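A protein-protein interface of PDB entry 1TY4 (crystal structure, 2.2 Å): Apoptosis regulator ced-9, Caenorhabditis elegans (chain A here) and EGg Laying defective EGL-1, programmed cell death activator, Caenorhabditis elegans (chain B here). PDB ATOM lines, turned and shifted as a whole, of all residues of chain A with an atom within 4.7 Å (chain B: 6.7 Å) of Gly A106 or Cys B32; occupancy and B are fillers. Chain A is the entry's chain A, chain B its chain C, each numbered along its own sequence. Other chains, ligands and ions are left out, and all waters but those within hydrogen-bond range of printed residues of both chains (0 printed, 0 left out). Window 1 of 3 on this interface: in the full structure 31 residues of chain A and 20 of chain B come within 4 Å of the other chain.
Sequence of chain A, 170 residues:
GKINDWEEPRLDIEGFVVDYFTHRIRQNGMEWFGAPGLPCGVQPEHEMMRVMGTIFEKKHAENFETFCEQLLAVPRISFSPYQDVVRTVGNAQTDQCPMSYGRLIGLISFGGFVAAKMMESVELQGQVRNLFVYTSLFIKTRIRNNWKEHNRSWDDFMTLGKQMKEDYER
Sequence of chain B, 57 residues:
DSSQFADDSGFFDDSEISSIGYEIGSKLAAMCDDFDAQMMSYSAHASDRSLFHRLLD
N of Gly A102 sits at hydrogen-bond distance from OD1 of Asp B36 (3.1 Å).
The guanidinium group of Arg A103 is in salt-bridge range of the side-chain carboxylate of Asp B33, at 2.9 Å.
The side-chain sulfur of Cys B32 lies close to the backbone carbonyl oxygen of Gly A102, at 3.6 Å.
Printed residues of chain B within 4 Å of Gly A102: Cys B32 (3.5 Å), Asp B36 (3.1 Å) and Met B39 (3.6 Å).
Of chain B, only Cys B32 comes within 4 Å of Gly A106.
Of the printed residues of chain A, Ala B29 touches Val A89 (3.9 Å).
Ala B30 touches none of the printed residues of chain A.
Cys B32 touches three residues of chain A.
Of the printed residues of chain A, Met B39 touches Gly A102 and Ile A105.
The nearest residue of chain B that does not touch Gly A106 is Leu B28 (4.2 Å).
Met B31 touches Phe A56.
CD1 of Phe A56 touches CD1 of Phe B35, at 3.5 Å.
CG2 of Val A89 touches CB of Leu B28, at 3.7 Å.
CG2 of Val A89 touches N of Ala B29 (3.9 Å).
Met B39 touches Gly A102 (CE to N, 3.6 Å).
Arg A103 touches Cys B32.
CE2 of Phe B35 touches CD1 of Ile A105, 3.7 Å away.
CD1 of Ile A105 touches SD of Met B39, 3.6 Å away.
Cys B32 touches Gly A106.
CD2 of Phe A110 touches CD1 of Leu B28, 3.9 Å away.
NH1 of Arg A103 is in hydrogen-bond range of O of Val A89 (3.1 Å).
The backbone carbonyl oxygen of Leu B28 sits at hydrogen-bond distance from the side-chain sulfur of Cys B32 (2.7 Å).
Of the 12 printed residues of chain B, 8 touch a printed residue of chain A.
Of the 12 printed residues of chain A, 7 touch a printed residue of chain B.
Hydrophobic or aromatic side chains of chain A that line the printed part of chain B: Phe A56, Val A89, Ile A105 and Phe A110.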
ATOM      1  N   PHE A  56     -22.402  27.685   0.062  1.00  0.00           N
ATOM      2  CA  PHE A  56     -22.741  28.115  -1.283  1.00  0.00           C
ATOM      3  C   PHE A  56     -24.243  28.003  -1.565  1.00  0.00           C
ATOM      4  O   PHE A  56     -24.858  28.936  -2.092  1.00  0.00           O
ATOM      5  CB  PHE A  56     -21.963  27.285  -2.306  1.00  0.00           C
ATOM      6  CG  PHE A  56     -22.013  27.840  -3.689  1.00  0.00           C
ATOM      7  CD1 PHE A  56     -21.033  28.723  -4.131  1.00  0.00           C
ATOM      8  CD2 PHE A  56     -23.059  27.512  -4.545  1.00  0.00           C
ATOM      9  CE1 PHE A  56     -21.095  29.275  -5.405  1.00  0.00           C
ATOM     10  CE2 PHE A  56     -23.133  28.058  -5.823  1.00  0.00           C
ATOM     11  CZ  PHE A  56     -22.152  28.942  -6.257  1.00  0.00           C
ATOM     12  N   VAL A  89     -20.158  26.921 -17.261  1.00  0.00           N
ATOM     13  CA  VAL A  89     -19.429  27.402 -16.093  1.00  0.00           C
ATOM     14  C   VAL A  89     -17.927  27.262 -16.318  1.00  0.00           C
ATOM     15  O   VAL A  89     -17.156  28.169 -16.007  1.00  0.00           O
ATOM     16  CB  VAL A  89     -19.812  26.634 -14.818  1.00  0.00           C
ATOM     17  CG1 VAL A  89     -18.800  26.928 -13.715  1.00  0.00           C
ATOM     18  CG2 VAL A  89     -21.209  27.048 -14.362  1.00  0.00           C
ATOM     19  N   GLY A 102     -14.013  28.488  -6.509  1.00  0.00           N
ATOM     20  CA  GLY A 102     -15.403  28.916  -6.570  1.00  0.00           C
ATOM     21  C   GLY A 102     -16.254  28.149  -7.578  1.00  0.00           C
ATOM     22  O   GLY A 102     -17.398  27.810  -7.299  1.00  0.00           O
ATOM     23  N   ARG A 103     -15.704  27.892  -8.757  1.00  0.00           N
ATOM     24  CA  ARG A 103     -16.428  27.160  -9.778  1.00  0.00           C
ATOM     25  C   ARG A 103     -16.533  25.685  -9.407  1.00  0.00           C
ATOM     26  O   ARG A 103     -17.536  25.035  -9.685  1.00  0.00           O
ATOM     27  CB  ARG A 103     -15.739  27.352 -11.122  1.00  0.00           C
ATOM     28  CG  ARG A 103     -15.956  28.756 -11.648  1.00  0.00           C
ATOM     29  CD  ARG A 103     -15.283  28.982 -12.980  1.00  0.00           C
ATOM     30  NE  ARG A 103     -15.460  30.361 -13.418  1.00  0.00           N
ATOM     31  CZ  ARG A 103     -15.181  30.796 -14.641  1.00  0.00           C
ATOM     32  NH1 ARG A 103     -14.712  29.954 -15.556  1.00  0.00           N
ATOM     33  NH2 ARG A 103     -15.361  32.076 -14.947  1.00  0.00           N
ATOM     34  N   LEU A 104     -15.494  25.173  -8.760  1.00  0.00           N
ATOM     35  CA  LEU A 104     -15.471  23.794  -8.314  1.00  0.00           C
ATOM     36  C   LEU A 104     -16.593  23.623  -7.283  1.00  0.00           C
ATOM     37  O   LEU A 104     -17.413  22.709  -7.376  1.00  0.00           O
ATOM     38  CB  LEU A 104     -14.116  23.485  -7.671  1.00  0.00           C
ATOM     39  CG  LEU A 104     -13.886  22.082  -7.099  1.00  0.00           C
ATOM     40  CD1 LEU A 104     -13.903  21.069  -8.221  1.00  0.00           C
ATOM     41  CD2 LEU A 104     -12.545  22.037  -6.381  1.00  0.00           C
ATOM     42  N   ILE A 105     -16.622  24.519  -6.301  1.00  0.00           N
ATOM     43  CA  ILE A 105     -17.635  24.470  -5.253  1.00  0.00           C
ATOM     44  C   ILE A 105     -19.041  24.680  -5.825  1.00  0.00           C
ATOM     45  O   ILE A 105     -19.989  24.010  -5.420  1.00  0.00           O
ATOM     46  CB  ILE A 105     -17.355  25.543  -4.171  1.00  0.00           C
ATOM     47  CG1 ILE A 105     -16.027  25.233  -3.479  1.00  0.00           C
ATOM     48  CG2 ILE A 105     -18.491  25.575  -3.145  1.00  0.00           C
ATOM     49  CD1 ILE A 105     -15.393  26.436  -2.777  1.00  0.00           C
ATOM     50  N   GLY A 106     -19.162  25.611  -6.765  1.00  0.00           N
ATOM     51  CA  GLY A 106     -20.450  25.892  -7.375  1.00  0.00           C
ATOM     52  C   GLY A 106     -21.027  24.699  -8.117  1.00  0.00           C
ATOM     53  O   GLY A 106     -22.206  24.377  -7.966  1.00  0.00           O
ATOM     54  N   LEU A 107     -20.189  24.044  -8.919  1.00  0.00           N
ATOM     55  CA  LEU A 107     -20.601  22.878  -9.687  1.00  0.00           C
ATOM     56  C   LEU A 107     -20.949  21.698  -8.785  1.00  0.00           C
ATOM     57  O   LEU A 107     -21.946  21.003  -9.006  1.00  0.00           O
ATOM     58  CB  LEU A 107     -19.493  22.480 -10.660  1.00  0.00           C
ATOM     59  CG  LEU A 107     -19.249  23.443 -11.836  1.00  0.00           C
ATOM     60  CD1 LEU A 107     -18.047  22.978 -12.650  1.00  0.00           C
ATOM     61  CD2 LEU A 107     -20.488  23.511 -12.723  1.00  0.00           C
ATOM     62  N   ILE A 108     -20.143  21.460  -7.757  1.00  0.00           N
ATOM     63  CA  ILE A 108     -20.432  20.346  -6.877  1.00  0.00           C
ATOM     64  C   ILE A 108     -21.642  20.654  -5.987  1.00  0.00           C
ATOM     65  O   ILE A 108     -22.469  19.774  -5.727  1.00  0.00           O
ATOM     66  CB  ILE A 108     -19.187  19.972  -6.043  1.00  0.00           C
ATOM     67  CG1 ILE A 108     -18.127  19.360  -6.971  1.00  0.00           C
ATOM     68  CG2 ILE A 108     -19.563  18.993  -4.937  1.00  0.00           C
ATOM     69  CD1 ILE A 108     -16.819  18.965  -6.286  1.00  0.00           C
ATOM     70  N   SER A 109     -21.775  21.904  -5.550  1.00  0.00           N
ATOM     71  CA  SER A 109     -22.917  22.278  -4.713  1.00  0.00           C
ATOM     72  C   SER A 109     -24.234  22.183  -5.498  1.00  0.00           C
ATOM     73  O   SER A 109     -25.218  21.642  -5.002  1.00  0.00           O
ATOM     74  CB  SER A 109     -22.753  23.703  -4.166  1.00  0.00           C
ATOM     75  OG  SER A 109     -23.888  24.080  -3.388  1.00  0.00           O
ATOM     76  N   PHE A 110     -24.260  22.710  -6.719  1.00  0.00           N
ATOM     77  CA  PHE A 110     -25.482  22.644  -7.524  1.00  0.00           C
ATOM     78  C   PHE A 110     -25.776  21.195  -7.919  1.00  0.00           C
ATOM     79  O   PHE A 110     -26.921  20.734  -7.822  1.00  0.00           O
ATOM     80  CB  PHE A 110     -25.353  23.508  -8.785  1.00  0.00           C
ATOM     81  CG  PHE A 110     -26.599  23.518  -9.647  1.00  0.00           C
ATOM     82  CD1 PHE A 110     -27.826  23.931  -9.121  1.00  0.00           C
ATOM     83  CD2 PHE A 110     -26.553  23.091 -10.969  1.00  0.00           C
ATOM     84  CE1 PHE A 110     -28.993  23.915  -9.907  1.00  0.00           C
ATOM     85  CE2 PHE A 110     -27.711  23.070 -11.763  1.00  0.00           C
ATOM     86  CZ  PHE A 110     -28.928  23.481 -11.230  1.00  0.00           C
ATOM     87  N   GLY A 111     -24.741  20.483  -8.367  1.00  0.00           N
ATOM     88  CA  GLY A 111     -24.905  19.093  -8.761  1.00  0.00           C
ATOM     89  C   GLY A 111     -25.455  18.245  -7.623  1.00  0.00           C
ATOM     90  O   GLY A 111     -26.275  17.358  -7.842  1.00  0.00           O
ATOM     91  N   LYS B  27     -25.411  32.300 -15.015  1.00  0.00           N
ATOM     92  CA  LYS B  27     -25.702  32.764 -13.664  1.00  0.00           C
ATOM     93  C   LYS B  27     -24.869  32.006 -12.639  1.00  0.00           C
ATOM     94  O   LYS B  27     -24.354  32.602 -11.692  1.00  0.00           O
ATOM     95  CB  LYS B  27     -27.192  32.593 -13.343  1.00  0.00           C
ATOM     96  CG  LYS B  27     -28.118  33.383 -14.268  1.00  0.00           C
ATOM     97  CD  LYS B  27     -29.581  33.218 -13.872  1.00  0.00           C
ATOM     98  CE  LYS B  27     -30.495  34.026 -14.784  1.00  0.00           C
ATOM     99  NZ  LYS B  27     -31.930  33.893 -14.396  1.00  0.00           N
ATOM    100  N   LEU B  28     -24.743  30.691 -12.826  1.00  0.00           N
ATOM    101  CA  LEU B  28     -23.973  29.862 -11.903  1.00  0.00           C
ATOM    102  C   LEU B  28     -22.525  30.325 -11.870  1.00  0.00           C
ATOM    103  O   LEU B  28     -21.913  30.391 -10.801  1.00  0.00           O
ATOM    104  CB  LEU B  28     -24.000  28.384 -12.326  1.00  0.00           C
ATOM    105  CG  LEU B  28     -24.471  27.359 -11.288  1.00  0.00           C
ATOM    106  CD1 LEU B  28     -24.006  25.965 -11.704  1.00  0.00           C
ATOM    107  CD2 LEU B  28     -23.917  27.707  -9.906  1.00  0.00           C
ATOM    108  N   ALA B  29     -21.988  30.636 -13.045  1.00  0.00           N
ATOM    109  CA  ALA B  29     -20.609  31.085 -13.176  1.00  0.00           C
ATOM    110  C   ALA B  29     -20.375  32.410 -12.448  1.00  0.00           C
ATOM    111  O   ALA B  29     -19.337  32.591 -11.803  1.00  0.00           O
ATOM    112  CB  ALA B  29     -20.237  31.213 -14.658  1.00  0.00           C
ATOM    113  N   ALA B  30     -21.334  33.331 -12.545  1.00  0.00           N
ATOM    114  CA  ALA B  30     -21.206  34.620 -11.858  1.00  0.00           C
ATOM    115  C   ALA B  30     -21.230  34.360 -10.350  1.00  0.00           C
ATOM    116  O   ALA B  30     -20.388  34.869  -9.607  1.00  0.00           O
ATOM    117  CB  ALA B  30     -22.347  35.556 -12.256  1.00  0.00           C
ATOM    118  N   MET B  31     -22.192  33.557  -9.904  1.00  0.00           N
ATOM    119  CA  MET B  31     -22.298  33.208  -8.489  1.00  0.00           C
ATOM    120  C   MET B  31     -20.995  32.543  -8.037  1.00  0.00           C
ATOM    121  O   MET B  31     -20.476  32.827  -6.955  1.00  0.00           O
ATOM    122  CB  MET B  31     -23.453  32.225  -8.256  1.00  0.00           C
ATOM    123  CG  MET B  31     -24.855  32.778  -8.489  1.00  0.00           C
ATOM    124  SD  MET B  31     -26.180  31.343  -8.733  1.00  0.00           S
ATOM    125  CE  MET B  31     -25.473  30.032  -7.536  1.00  0.00           C
ATOM    126  N   CYS B  32     -20.477  31.654  -8.880  1.00  0.00           N
ATOM    127  CA  CYS B  32     -19.244  30.930  -8.585  1.00  0.00           C
ATOM    128  C   CYS B  32     -18.052  31.873  -8.456  1.00  0.00           C
ATOM    129  O   CYS B  32     -17.241  31.741  -7.544  1.00  0.00           O
ATOM    130  CB  CYS B  32     -18.971  29.887  -9.679  1.00  0.00           C
ATOM    131  SG  CYS B  32     -19.945  28.854  -9.654  1.00  0.00           S
ATOM    132  N   ASP B  33     -17.951  32.825  -9.376  1.00  0.00           N
ATOM    133  CA  ASP B  33     -16.859  33.780  -9.343  1.00  0.00           C
ATOM    134  C   ASP B  33     -16.967  34.702  -8.138  1.00  0.00           C
ATOM    135  O   ASP B  33     -15.951  35.095  -7.558  1.00  0.00           O
ATOM    136  CB  ASP B  33     -16.820  34.571 -10.651  1.00  0.00           C
ATOM    137  CG  ASP B  33     -16.441  33.696 -11.817  1.00  0.00           C
ATOM    138  OD1 ASP B  33     -15.928  32.585 -11.552  1.00  0.00           O
ATOM    139  OD2 ASP B  33     -16.637  34.104 -12.981  1.00  0.00           O
ATOM    140  N   ASP B  34     -18.193  35.039  -7.754  1.00  0.00           N
ATOM    141  CA  ASP B  34     -18.387  35.881  -6.585  1.00  0.00           C
ATOM    142  C   ASP B  34     -17.903  35.111  -5.355  1.00  0.00           C
ATOM    143  O   ASP B  34     -17.259  35.684  -4.481  1.00  0.00           O
ATOM    144  CB  ASP B  34     -19.861  36.265  -6.410  1.00  0.00           C
ATOM    145  CG  ASP B  34     -20.327  37.313  -7.417  1.00  0.00           C
ATOM    146  OD1 ASP B  34     -19.491  37.830  -8.189  1.00  0.00           O
ATOM    147  OD2 ASP B  34     -21.538  37.625  -7.431  1.00  0.00           O
ATOM    148  N   PHE B  35     -18.205  33.813  -5.283  1.00  0.00           N
ATOM    149  CA  PHE B  35     -17.767  33.008  -4.139  1.00  0.00           C
ATOM    150  C   PHE B  35     -16.240  32.915  -4.109  1.00  0.00           C
ATOM    151  O   PHE B  35     -15.625  33.021  -3.049  1.00  0.00           O
ATOM    152  CB  PHE B  35     -18.340  31.591  -4.210  1.00  0.00           C
ATOM    153  CG  PHE B  35     -18.283  30.847  -2.903  1.00  0.00           C
ATOM    154  CD1 PHE B  35     -19.342  30.912  -2.008  1.00  0.00           C
ATOM    155  CD2 PHE B  35     -17.174  30.079  -2.568  1.00  0.00           C
ATOM    156  CE1 PHE B  35     -19.302  30.220  -0.795  1.00  0.00           C
ATOM    157  CE2 PHE B  35     -17.120  29.384  -1.360  1.00  0.00           C
ATOM    158  CZ  PHE B  35     -18.188  29.453  -0.473  1.00  0.00           C
ATOM    159  N   ASP B  36     -15.642  32.704  -5.280  1.00  0.00           N
ATOM    160  CA  ASP B  36     -14.195  32.588  -5.402  1.00  0.00           C
ATOM    161  C   ASP B  36     -13.514  33.881  -4.947  1.00  0.00           C
ATOM    162  O   ASP B  36     -12.554  33.852  -4.175  1.00  0.00           O
ATOM    163  CB  ASP B  36     -13.815  32.283  -6.850  1.00  0.00           C
ATOM    164  CG  ASP B  36     -12.358  31.875  -6.999  1.00  0.00           C
ATOM    165  OD1 ASP B  36     -11.957  30.860  -6.385  1.00  0.00           O
ATOM    166  OD2 ASP B  36     -11.614  32.565  -7.733  1.00  0.00           O
ATOM    167  N   ALA B  37     -14.022  35.014  -5.427  1.00  0.00           N
ATOM    168  CA  ALA B  37     -13.469  36.312  -5.062  1.00  0.00           C
ATOM    169  C   ALA B  37     -13.431  36.462  -3.542  1.00  0.00           C
ATOM    170  O   ALA B  37     -12.409  36.847  -2.973  1.00  0.00           O
ATOM    171  CB  ALA B  37     -14.306  37.428  -5.681  1.00  0.00           C
ATOM    172  N   MET B  39     -13.637  34.063  -1.147  1.00  0.00           N
ATOM    173  CA  MET B  39     -12.754  33.056  -0.576  1.00  0.00           C
ATOM    174  C   MET B  39     -11.288  33.425  -0.812  1.00  0.00           C
ATOM    175  O   MET B  39     -10.440  33.202   0.042  1.00  0.00           O
ATOM    176  CB  MET B  39     -13.078  31.693  -1.205  1.00  0.00           C
ATOM    177  CG  MET B  39     -12.392  30.476  -0.586  1.00  0.00           C
ATOM    178  SD  MET B  39     -12.970  28.817  -1.479  1.00  0.00           S
ATOM    179  CE  MET B  39     -12.949  29.515  -3.268  1.00  0.00           C
